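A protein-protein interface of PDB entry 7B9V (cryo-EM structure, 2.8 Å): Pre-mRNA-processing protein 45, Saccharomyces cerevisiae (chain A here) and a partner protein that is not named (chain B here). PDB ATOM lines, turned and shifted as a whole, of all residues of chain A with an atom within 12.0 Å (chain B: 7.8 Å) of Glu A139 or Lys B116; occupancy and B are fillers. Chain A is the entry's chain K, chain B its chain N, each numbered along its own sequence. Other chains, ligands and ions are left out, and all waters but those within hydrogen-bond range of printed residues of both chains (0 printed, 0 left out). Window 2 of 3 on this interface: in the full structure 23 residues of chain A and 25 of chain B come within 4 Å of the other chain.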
ATOM      1  N   VAL A 134      39.077  20.040  16.590  1.00  0.00           N
ATOM      2  CA  VAL A 134      37.792  20.256  15.923  1.00  0.00           C
ATOM      3  C   VAL A 134      37.051  21.376  16.651  1.00  0.00           C
ATOM      4  O   VAL A 134      36.989  21.383  17.885  1.00  0.00           O
ATOM      5  CB  VAL A 134      36.909  18.978  15.925  1.00  0.00           C
ATOM      6  CG1 VAL A 134      35.627  19.219  15.209  1.00  0.00           C
ATOM      7  CG2 VAL A 134      37.561  17.754  15.262  1.00  0.00           C
ATOM      8  N   VAL A 135      36.500  22.326  15.895  1.00  0.00           N
ATOM      9  CA  VAL A 135      35.536  23.287  16.420  1.00  0.00           C
ATOM     10  C   VAL A 135      34.138  22.747  16.136  1.00  0.00           C
ATOM     11  O   VAL A 135      33.750  22.601  14.973  1.00  0.00           O
ATOM     12  CB  VAL A 135      35.722  24.670  15.786  1.00  0.00           C
ATOM     13  CG1 VAL A 135      34.620  25.619  16.224  1.00  0.00           C
ATOM     14  CG2 VAL A 135      37.049  25.224  16.171  1.00  0.00           C
ATOM     15  N   ALA A 136      33.397  22.426  17.189  1.00  0.00           N
ATOM     16  CA  ALA A 136      32.080  21.815  17.040  1.00  0.00           C
ATOM     17  C   ALA A 136      31.025  22.891  16.801  1.00  0.00           C
ATOM     18  O   ALA A 136      31.059  23.931  17.467  1.00  0.00           O
ATOM     19  CB  ALA A 136      31.719  20.994  18.273  1.00  0.00           C
ATOM     20  N   PRO A 137      30.111  22.708  15.842  1.00  0.00           N
ATOM     21  CA  PRO A 137      29.020  23.677  15.676  1.00  0.00           C
ATOM     22  C   PRO A 137      28.025  23.603  16.817  1.00  0.00           C
ATOM     23  O   PRO A 137      27.586  22.523  17.212  1.00  0.00           O
ATOM     24  CB  PRO A 137      28.356  23.263  14.357  1.00  0.00           C
ATOM     25  CG  PRO A 137      29.262  22.405  13.737  1.00  0.00           C
ATOM     26  CD  PRO A 137      30.049  21.696  14.789  1.00  0.00           C
ATOM     27  N   THR A 138      27.666  24.770  17.328  1.00  0.00           N
ATOM     28  CA  THR A 138      26.647  24.894  18.359  1.00  0.00           C
ATOM     29  C   THR A 138      25.318  25.221  17.679  1.00  0.00           C
ATOM     30  O   THR A 138      24.855  26.362  17.664  1.00  0.00           O
ATOM     31  CB  THR A 138      27.059  25.943  19.384  1.00  0.00           C
ATOM     32  OG1 THR A 138      27.370  27.164  18.708  1.00  0.00           O
ATOM     33  CG2 THR A 138      28.278  25.474  20.161  1.00  0.00           C
ATOM     34  N   GLU A 139      24.702  24.191  17.098  1.00  0.00           N
ATOM     35  CA  GLU A 139      23.403  24.329  16.456  1.00  0.00           C
ATOM     36  C   GLU A 139      22.307  23.998  17.460  1.00  0.00           C
ATOM     37  O   GLU A 139      22.436  23.058  18.250  1.00  0.00           O
ATOM     38  CB  GLU A 139      23.296  23.416  15.231  1.00  0.00           C
ATOM     39  CG  GLU A 139      24.433  23.571  14.234  1.00  0.00           C
ATOM     40  CD  GLU A 139      24.595  25.002  13.746  1.00  0.00           C
ATOM     41  OE1 GLU A 139      23.577  25.629  13.378  1.00  0.00           O
ATOM     42  OE2 GLU A 139      25.738  25.502  13.730  1.00  0.00           O
ATOM     43  N   ASN A 140      21.222  24.773  17.414  1.00  0.00           N
ATOM     44  CA  ASN A 140      20.114  24.605  18.355  1.00  0.00           C
ATOM     45  C   ASN A 140      18.882  25.255  17.744  1.00  0.00           C
ATOM     46  O   ASN A 140      18.918  26.439  17.394  1.00  0.00           O
ATOM     47  CB  ASN A 140      20.443  25.232  19.723  1.00  0.00           C
ATOM     48  CG  ASN A 140      19.246  25.272  20.675  1.00  0.00           C
ATOM     49  OD1 ASN A 140      18.361  24.411  20.641  1.00  0.00           O
ATOM     50  ND2 ASN A 140      19.214  26.289  21.526  1.00  0.00           N
ATOM     51  N   ASP A 141      17.801  24.485  17.619  1.00  0.00           N
ATOM     52  CA  ASP A 141      16.563  24.981  17.032  1.00  0.00           C
ATOM     53  C   ASP A 141      15.682  25.705  18.047  1.00  0.00           C
ATOM     54  O   ASP A 141      14.840  26.514  17.640  1.00  0.00           O
ATOM     55  CB  ASP A 141      15.775  23.825  16.406  1.00  0.00           C
ATOM     56  CG  ASP A 141      16.493  23.198  15.230  1.00  0.00           C
ATOM     57  OD1 ASP A 141      17.204  23.932  14.513  1.00  0.00           O
ATOM     58  OD2 ASP A 141      16.341  21.976  15.020  1.00  0.00           O
ATOM     59  N   GLU A 142      15.850  25.436  19.343  1.00  0.00           N
ATOM     60  CA  GLU A 142      14.929  25.882  20.389  1.00  0.00           C
ATOM     61  C   GLU A 142      15.528  27.053  21.163  1.00  0.00           C
ATOM     62  O   GLU A 142      16.618  26.935  21.733  1.00  0.00           O
ATOM     63  CB  GLU A 142      14.577  24.731  21.332  1.00  0.00           C
ATOM     64  CG  GLU A 142      13.804  23.580  20.680  1.00  0.00           C
ATOM     65  CD  GLU A 142      12.362  23.918  20.256  1.00  0.00           C
ATOM     66  OE1 GLU A 142      11.813  24.994  20.596  1.00  0.00           O
ATOM     67  OE2 GLU A 142      11.768  23.085  19.539  1.00  0.00           O
ATOM     68  N   VAL A 143      14.815  28.173  21.184  1.00  0.00           N
ATOM     69  CA  VAL A 143      15.226  29.328  21.977  1.00  0.00           C
ATOM     70  C   VAL A 143      14.780  29.146  23.434  1.00  0.00           C
ATOM     71  O   VAL A 143      13.670  28.673  23.712  1.00  0.00           O
ATOM     72  CB  VAL A 143      14.706  30.628  21.320  1.00  0.00           C
ATOM     73  CG1 VAL A 143      13.190  30.692  21.220  1.00  0.00           C
ATOM     74  CG2 VAL A 143      15.226  31.844  22.025  1.00  0.00           C
ATOM     75  N   VAL A 144      15.681  29.437  24.360  1.00  0.00           N
ATOM     76  CA  VAL A 144      15.420  29.330  25.796  1.00  0.00           C
ATOM     77  C   VAL A 144      15.114  30.711  26.358  1.00  0.00           C
ATOM     78  O   VAL A 144      15.967  31.612  26.257  1.00  0.00           O
ATOM     79  CB  VAL A 144      16.613  28.693  26.523  1.00  0.00           C
ATOM     80  CG1 VAL A 144      16.366  28.668  28.010  1.00  0.00           C
ATOM     81  CG2 VAL A 144      16.846  27.291  25.986  1.00  0.00           C
ATOM     82  N   ARG B  63      27.804  10.469   8.223  1.00  0.00           N
ATOM     83  CA  ARG B  63      27.164  11.770   8.427  1.00  0.00           C
ATOM     84  C   ARG B  63      27.384  12.745   7.264  1.00  0.00           C
ATOM     85  O   ARG B  63      26.462  13.498   6.921  1.00  0.00           O
ATOM     86  CB  ARG B  63      27.621  12.343   9.776  1.00  0.00           C
ATOM     87  CG  ARG B  63      29.098  12.674   9.929  1.00  0.00           C
ATOM     88  CD  ARG B  63      29.317  13.480  11.206  1.00  0.00           C
ATOM     89  NE  ARG B  63      28.877  12.758  12.399  1.00  0.00           N
ATOM     90  CZ  ARG B  63      29.635  11.940  13.117  1.00  0.00           C
ATOM     91  NH1 ARG B  63      30.901  11.717  12.809  1.00  0.00           N
ATOM     92  NH2 ARG B  63      29.108  11.331  14.177  1.00  0.00           N
ATOM     93  N   THR B  66      24.688  11.248   4.688  1.00  0.00           N
ATOM     94  CA  THR B  66      23.324  11.721   4.959  1.00  0.00           C
ATOM     95  C   THR B  66      23.155  13.220   4.721  1.00  0.00           C
ATOM     96  O   THR B  66      22.064  13.650   4.319  1.00  0.00           O
ATOM     97  CB  THR B  66      22.885  11.366   6.385  1.00  0.00           C
ATOM     98  OG1 THR B  66      23.764  11.966   7.334  1.00  0.00           O
ATOM     99  CG2 THR B  66      22.826   9.854   6.572  1.00  0.00           C
ATOM    100  N   GLN B  67      24.176  14.037   5.049  1.00  0.00           N
ATOM    101  CA  GLN B  67      24.159  15.471   4.712  1.00  0.00           C
ATOM    102  C   GLN B  67      23.953  15.722   3.223  1.00  0.00           C
ATOM    103  O   GLN B  67      23.285  16.689   2.836  1.00  0.00           O
ATOM    104  CB  GLN B  67      25.455  16.155   5.124  1.00  0.00           C
ATOM    105  CG  GLN B  67      25.545  16.660   6.533  1.00  0.00           C
ATOM    106  CD  GLN B  67      26.837  17.429   6.723  1.00  0.00           C
ATOM    107  OE1 GLN B  67      27.783  17.259   5.965  1.00  0.00           O
ATOM    108  NE2 GLN B  67      26.878  18.270   7.742  1.00  0.00           N
ATOM    109  N   MET B 109      37.119  24.163   8.473  1.00  0.00           N
ATOM    110  CA  MET B 109      35.738  24.321   8.026  1.00  0.00           C
ATOM    111  C   MET B 109      35.163  23.007   7.510  1.00  0.00           C
ATOM    112  O   MET B 109      33.965  22.768   7.678  1.00  0.00           O
ATOM    113  CB  MET B 109      35.628  25.458   6.997  1.00  0.00           C
ATOM    114  CG  MET B 109      34.183  25.791   6.553  1.00  0.00           C
ATOM    115  SD  MET B 109      32.975  26.163   7.834  1.00  0.00           S
ATOM    116  CE  MET B 109      31.464  26.383   6.905  1.00  0.00           C
ATOM    117  N   LYS B 110      36.000  22.126   6.929  1.00  0.00           N
ATOM    118  CA  LYS B 110      35.549  20.781   6.551  1.00  0.00           C
ATOM    119  C   LYS B 110      35.121  19.974   7.765  1.00  0.00           C
ATOM    120  O   LYS B 110      34.082  19.298   7.732  1.00  0.00           O
ATOM    121  CB  LYS B 110      36.635  20.025   5.789  1.00  0.00           C
ATOM    122  CG  LYS B 110      36.877  20.501   4.377  1.00  0.00           C
ATOM    123  CD  LYS B 110      38.106  19.828   3.801  1.00  0.00           C
ATOM    124  CE  LYS B 110      38.608  20.535   2.560  1.00  0.00           C
ATOM    125  NZ  LYS B 110      40.010  20.152   2.243  1.00  0.00           N
ATOM    126  N   ARG B 111      35.920  20.024   8.835  1.00  0.00           N
ATOM    127  CA  ARG B 111      35.588  19.325  10.072  1.00  0.00           C
ATOM    128  C   ARG B 111      34.356  19.937  10.722  1.00  0.00           C
ATOM    129  O   ARG B 111      33.502  19.209  11.246  1.00  0.00           O
ATOM    130  CB  ARG B 111      36.774  19.356  11.034  1.00  0.00           C
ATOM    131  CG  ARG B 111      37.993  18.621  10.519  1.00  0.00           C
ATOM    132  CD  ARG B 111      39.220  18.877  11.375  1.00  0.00           C
ATOM    133  NE  ARG B 111      40.421  18.323  10.759  1.00  0.00           N
ATOM    134  CZ  ARG B 111      41.654  18.517  11.205  1.00  0.00           C
ATOM    135  NH1 ARG B 111      41.893  19.252  12.279  1.00  0.00           N
ATOM    136  NH2 ARG B 111      42.673  17.962  10.558  1.00  0.00           N
ATOM    137  N   PHE B 112      34.312  21.276  10.775  1.00  0.00           N
ATOM    138  CA  PHE B 112      33.181  22.005  11.339  1.00  0.00           C
ATOM    139  C   PHE B 112      31.884  21.673  10.604  1.00  0.00           C
ATOM    140  O   PHE B 112      30.895  21.311  11.239  1.00  0.00           O
ATOM    141  CB  PHE B 112      33.478  23.514  11.289  1.00  0.00           C
ATOM    142  CG  PHE B 112      32.324  24.410  11.723  1.00  0.00           C
ATOM    143  CD1 PHE B 112      32.167  24.743  13.059  1.00  0.00           C
ATOM    144  CD2 PHE B 112      31.445  24.972  10.793  1.00  0.00           C
ATOM    145  CE1 PHE B 112      31.137  25.569  13.465  1.00  0.00           C
ATOM    146  CE2 PHE B 112      30.409  25.789  11.195  1.00  0.00           C
ATOM    147  CZ  PHE B 112      30.255  26.090  12.533  1.00  0.00           C
ATOM    148  N   LEU B 113      31.890  21.753   9.256  1.00  0.00           N
ATOM    149  CA  LEU B 113      30.665  21.597   8.456  1.00  0.00           C
ATOM    150  C   LEU B 113      30.070  20.201   8.585  1.00  0.00           C
ATOM    151  O   LEU B 113      28.854  20.030   8.462  1.00  0.00           O
ATOM    152  CB  LEU B 113      30.917  21.946   6.984  1.00  0.00           C
ATOM    153  CG  LEU B 113      29.842  21.826   5.894  1.00  0.00           C
ATOM    154  CD1 LEU B 113      29.953  23.020   4.976  1.00  0.00           C
ATOM    155  CD2 LEU B 113      29.997  20.548   5.073  1.00  0.00           C
ATOM    156  N   SER B 114      30.916  19.184   8.761  1.00  0.00           N
ATOM    157  CA  SER B 114      30.425  17.814   8.768  1.00  0.00           C
ATOM    158  C   SER B 114      29.602  17.484  10.005  1.00  0.00           C
ATOM    159  O   SER B 114      28.785  16.561   9.959  1.00  0.00           O
ATOM    160  CB  SER B 114      31.591  16.853   8.669  1.00  0.00           C
ATOM    161  OG  SER B 114      32.336  16.820   9.873  1.00  0.00           O
ATOM    162  N   LEU B 115      29.797  18.220  11.102  1.00  0.00           N
ATOM    163  CA  LEU B 115      29.161  17.877  12.363  1.00  0.00           C
ATOM    164  C   LEU B 115      27.803  18.540  12.571  1.00  0.00           C
ATOM    165  O   LEU B 115      27.058  18.109  13.456  1.00  0.00           O
ATOM    166  CB  LEU B 115      30.081  18.225  13.530  1.00  0.00           C
ATOM    167  CG  LEU B 115      31.236  17.257  13.758  1.00  0.00           C
ATOM    168  CD1 LEU B 115      32.239  17.963  14.606  1.00  0.00           C
ATOM    169  CD2 LEU B 115      30.780  15.984  14.438  1.00  0.00           C
ATOM    170  N   LYS B 116      27.462  19.575  11.796  1.00  0.00           N
ATOM    171  CA  LYS B 116      26.139  20.187  11.896  1.00  0.00           C
ATOM    172  C   LYS B 116      25.123  19.332  11.151  1.00  0.00           C
ATOM    173  O   LYS B 116      25.325  18.970   9.987  1.00  0.00           O
ATOM    174  CB  LYS B 116      26.116  21.638  11.390  1.00  0.00           C
ATOM    175  CG  LYS B 116      26.774  21.914  10.059  1.00  0.00           C
ATOM    176  CD  LYS B 116      26.420  23.279   9.475  1.00  0.00           C
ATOM    177  CE  LYS B 116      26.871  24.414  10.369  1.00  0.00           C
ATOM    178  NZ  LYS B 116      26.563  25.737   9.762  1.00  0.00           N
ATOM    179  N   ASN B 117      24.043  18.978  11.844  1.00  0.00           N
ATOM    180  CA  ASN B 117      23.063  18.010  11.347  1.00  0.00           C
ATOM    181  C   ASN B 117      21.982  18.677  10.488  1.00  0.00           C
ATOM    182  O   ASN B 117      20.779  18.594  10.732  1.00  0.00           O
ATOM    183  CB  ASN B 117      22.461  17.231  12.518  1.00  0.00           C
ATOM    184  CG  ASN B 117      21.831  18.133  13.585  1.00  0.00           C
ATOM    185  OD1 ASN B 117      22.183  19.306  13.708  1.00  0.00           O
ATOM    186  ND2 ASN B 117      20.865  17.595  14.321  1.00  0.00           N
ATOM    187  N   VAL B 118      22.442  19.314   9.415  1.00  0.00           N
ATOM    188  CA  VAL B 118      21.551  19.973   8.474  1.00  0.00           C
ATOM    189  C   VAL B 118      21.941  19.569   7.051  1.00  0.00           C
ATOM    190  O   VAL B 118      23.128  19.488   6.714  1.00  0.00           O
ATOM    191  CB  VAL B 118      21.540  21.512   8.684  1.00  0.00           C
ATOM    192  CG1 VAL B 118      22.906  22.182   8.471  1.00  0.00           C
ATOM    193  CG2 VAL B 118      20.481  22.169   7.808  1.00  0.00           C
ATOM    194  N   LYS B 119      20.942  19.153   6.281  1.00  0.00           N
ATOM    195  CA  LYS B 119      21.139  18.708   4.908  1.00  0.00           C
ATOM    196  C   LYS B 119      21.523  19.880   4.001  1.00  0.00           C
ATOM    197  O   LYS B 119      21.192  21.040   4.269  1.00  0.00           O
ATOM    198  CB  LYS B 119      19.901  17.952   4.423  1.00  0.00           C
ATOM    199  CG  LYS B 119      19.882  16.512   4.985  1.00  0.00           C
ATOM    200  CD  LYS B 119      18.680  15.664   4.579  1.00  0.00           C
ATOM    201  CE  LYS B 119      17.441  15.952   5.411  1.00  0.00           C
ATOM    202  NZ  LYS B 119      17.504  15.319   6.764  1.00  0.00           N
ATOM    203  N   LEU B 120      22.239  19.565   2.919  1.00  0.00           N
ATOM    204  CA  LEU B 120      22.945  20.545   2.099  1.00  0.00           C
ATOM    205  C   LEU B 120      22.495  20.438   0.650  1.00  0.00           C
ATOM    206  O   LEU B 120      22.403  19.336   0.121  1.00  0.00           O
ATOM    207  CB  LEU B 120      24.455  20.317   2.169  1.00  0.00           C
ATOM    208  CG  LEU B 120      25.084  20.212   3.553  1.00  0.00           C
ATOM    209  CD1 LEU B 120      26.530  19.765   3.444  1.00  0.00           C
ATOM    210  CD2 LEU B 120      24.983  21.545   4.255  1.00  0.00           C
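Among the printed residues, merely in contact across the chains: Pro A137 with Phe B112 (3.2 Å), Val A135 with Phe B112 (3.3 Å), Val A134 with Leu B115 (3.7 Å), Pro A137 with Leu B115 (3.7 Å), Glu A139 with Lys B116 (3.7 Å) and Pro A137 with Lys B116 (3.9 Å).
Among the printed residues, 6 pairs touch across the chains. Among the printed residues, no Asp or Glu carboxylate lies within 4 Å of a Lys or Arg side-chain nitrogen of the other chain.
Of the printed residues of chain B, Glu A139 touches Lys B116. Of chain A, only Pro A137 (3.9 Å) and Glu A139 (3.7 Å) come within 4 Å of Lys B116. Gln B67 touches none of the printed residues of chain A. Phe B112 touches just these residues of chain A: Val A135 (3.3 Å) and Pro A137 (3.2 Å). No residue of chain A comes within 4 Å of Ser B114. Of the printed residues of chain B, Pro A137 touches Phe B112 (3.2 Å), Leu B115 (3.7 Å) and Lys B116 (3.9 Å). Of the printed residues of chain B, Val A135 touches Phe B112 (3.3 Å). Arg B111 touches none of the printed residues of chain A. Arg B63 touches none of the printed residues of chain A. The nearest residue of chain B that does not touch Glu A139 is Asn B117 (4.5 Å). The nearest printed residue of chain B that does not touch Val A134 is Arg B111 (4.3 Å).
The backbone carbonyl oxygen (O) of Lys B116 is in hydrogen-bond range of the side-chain amide nitrogen (NE2) of Gln B67, 2.8 Å away.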
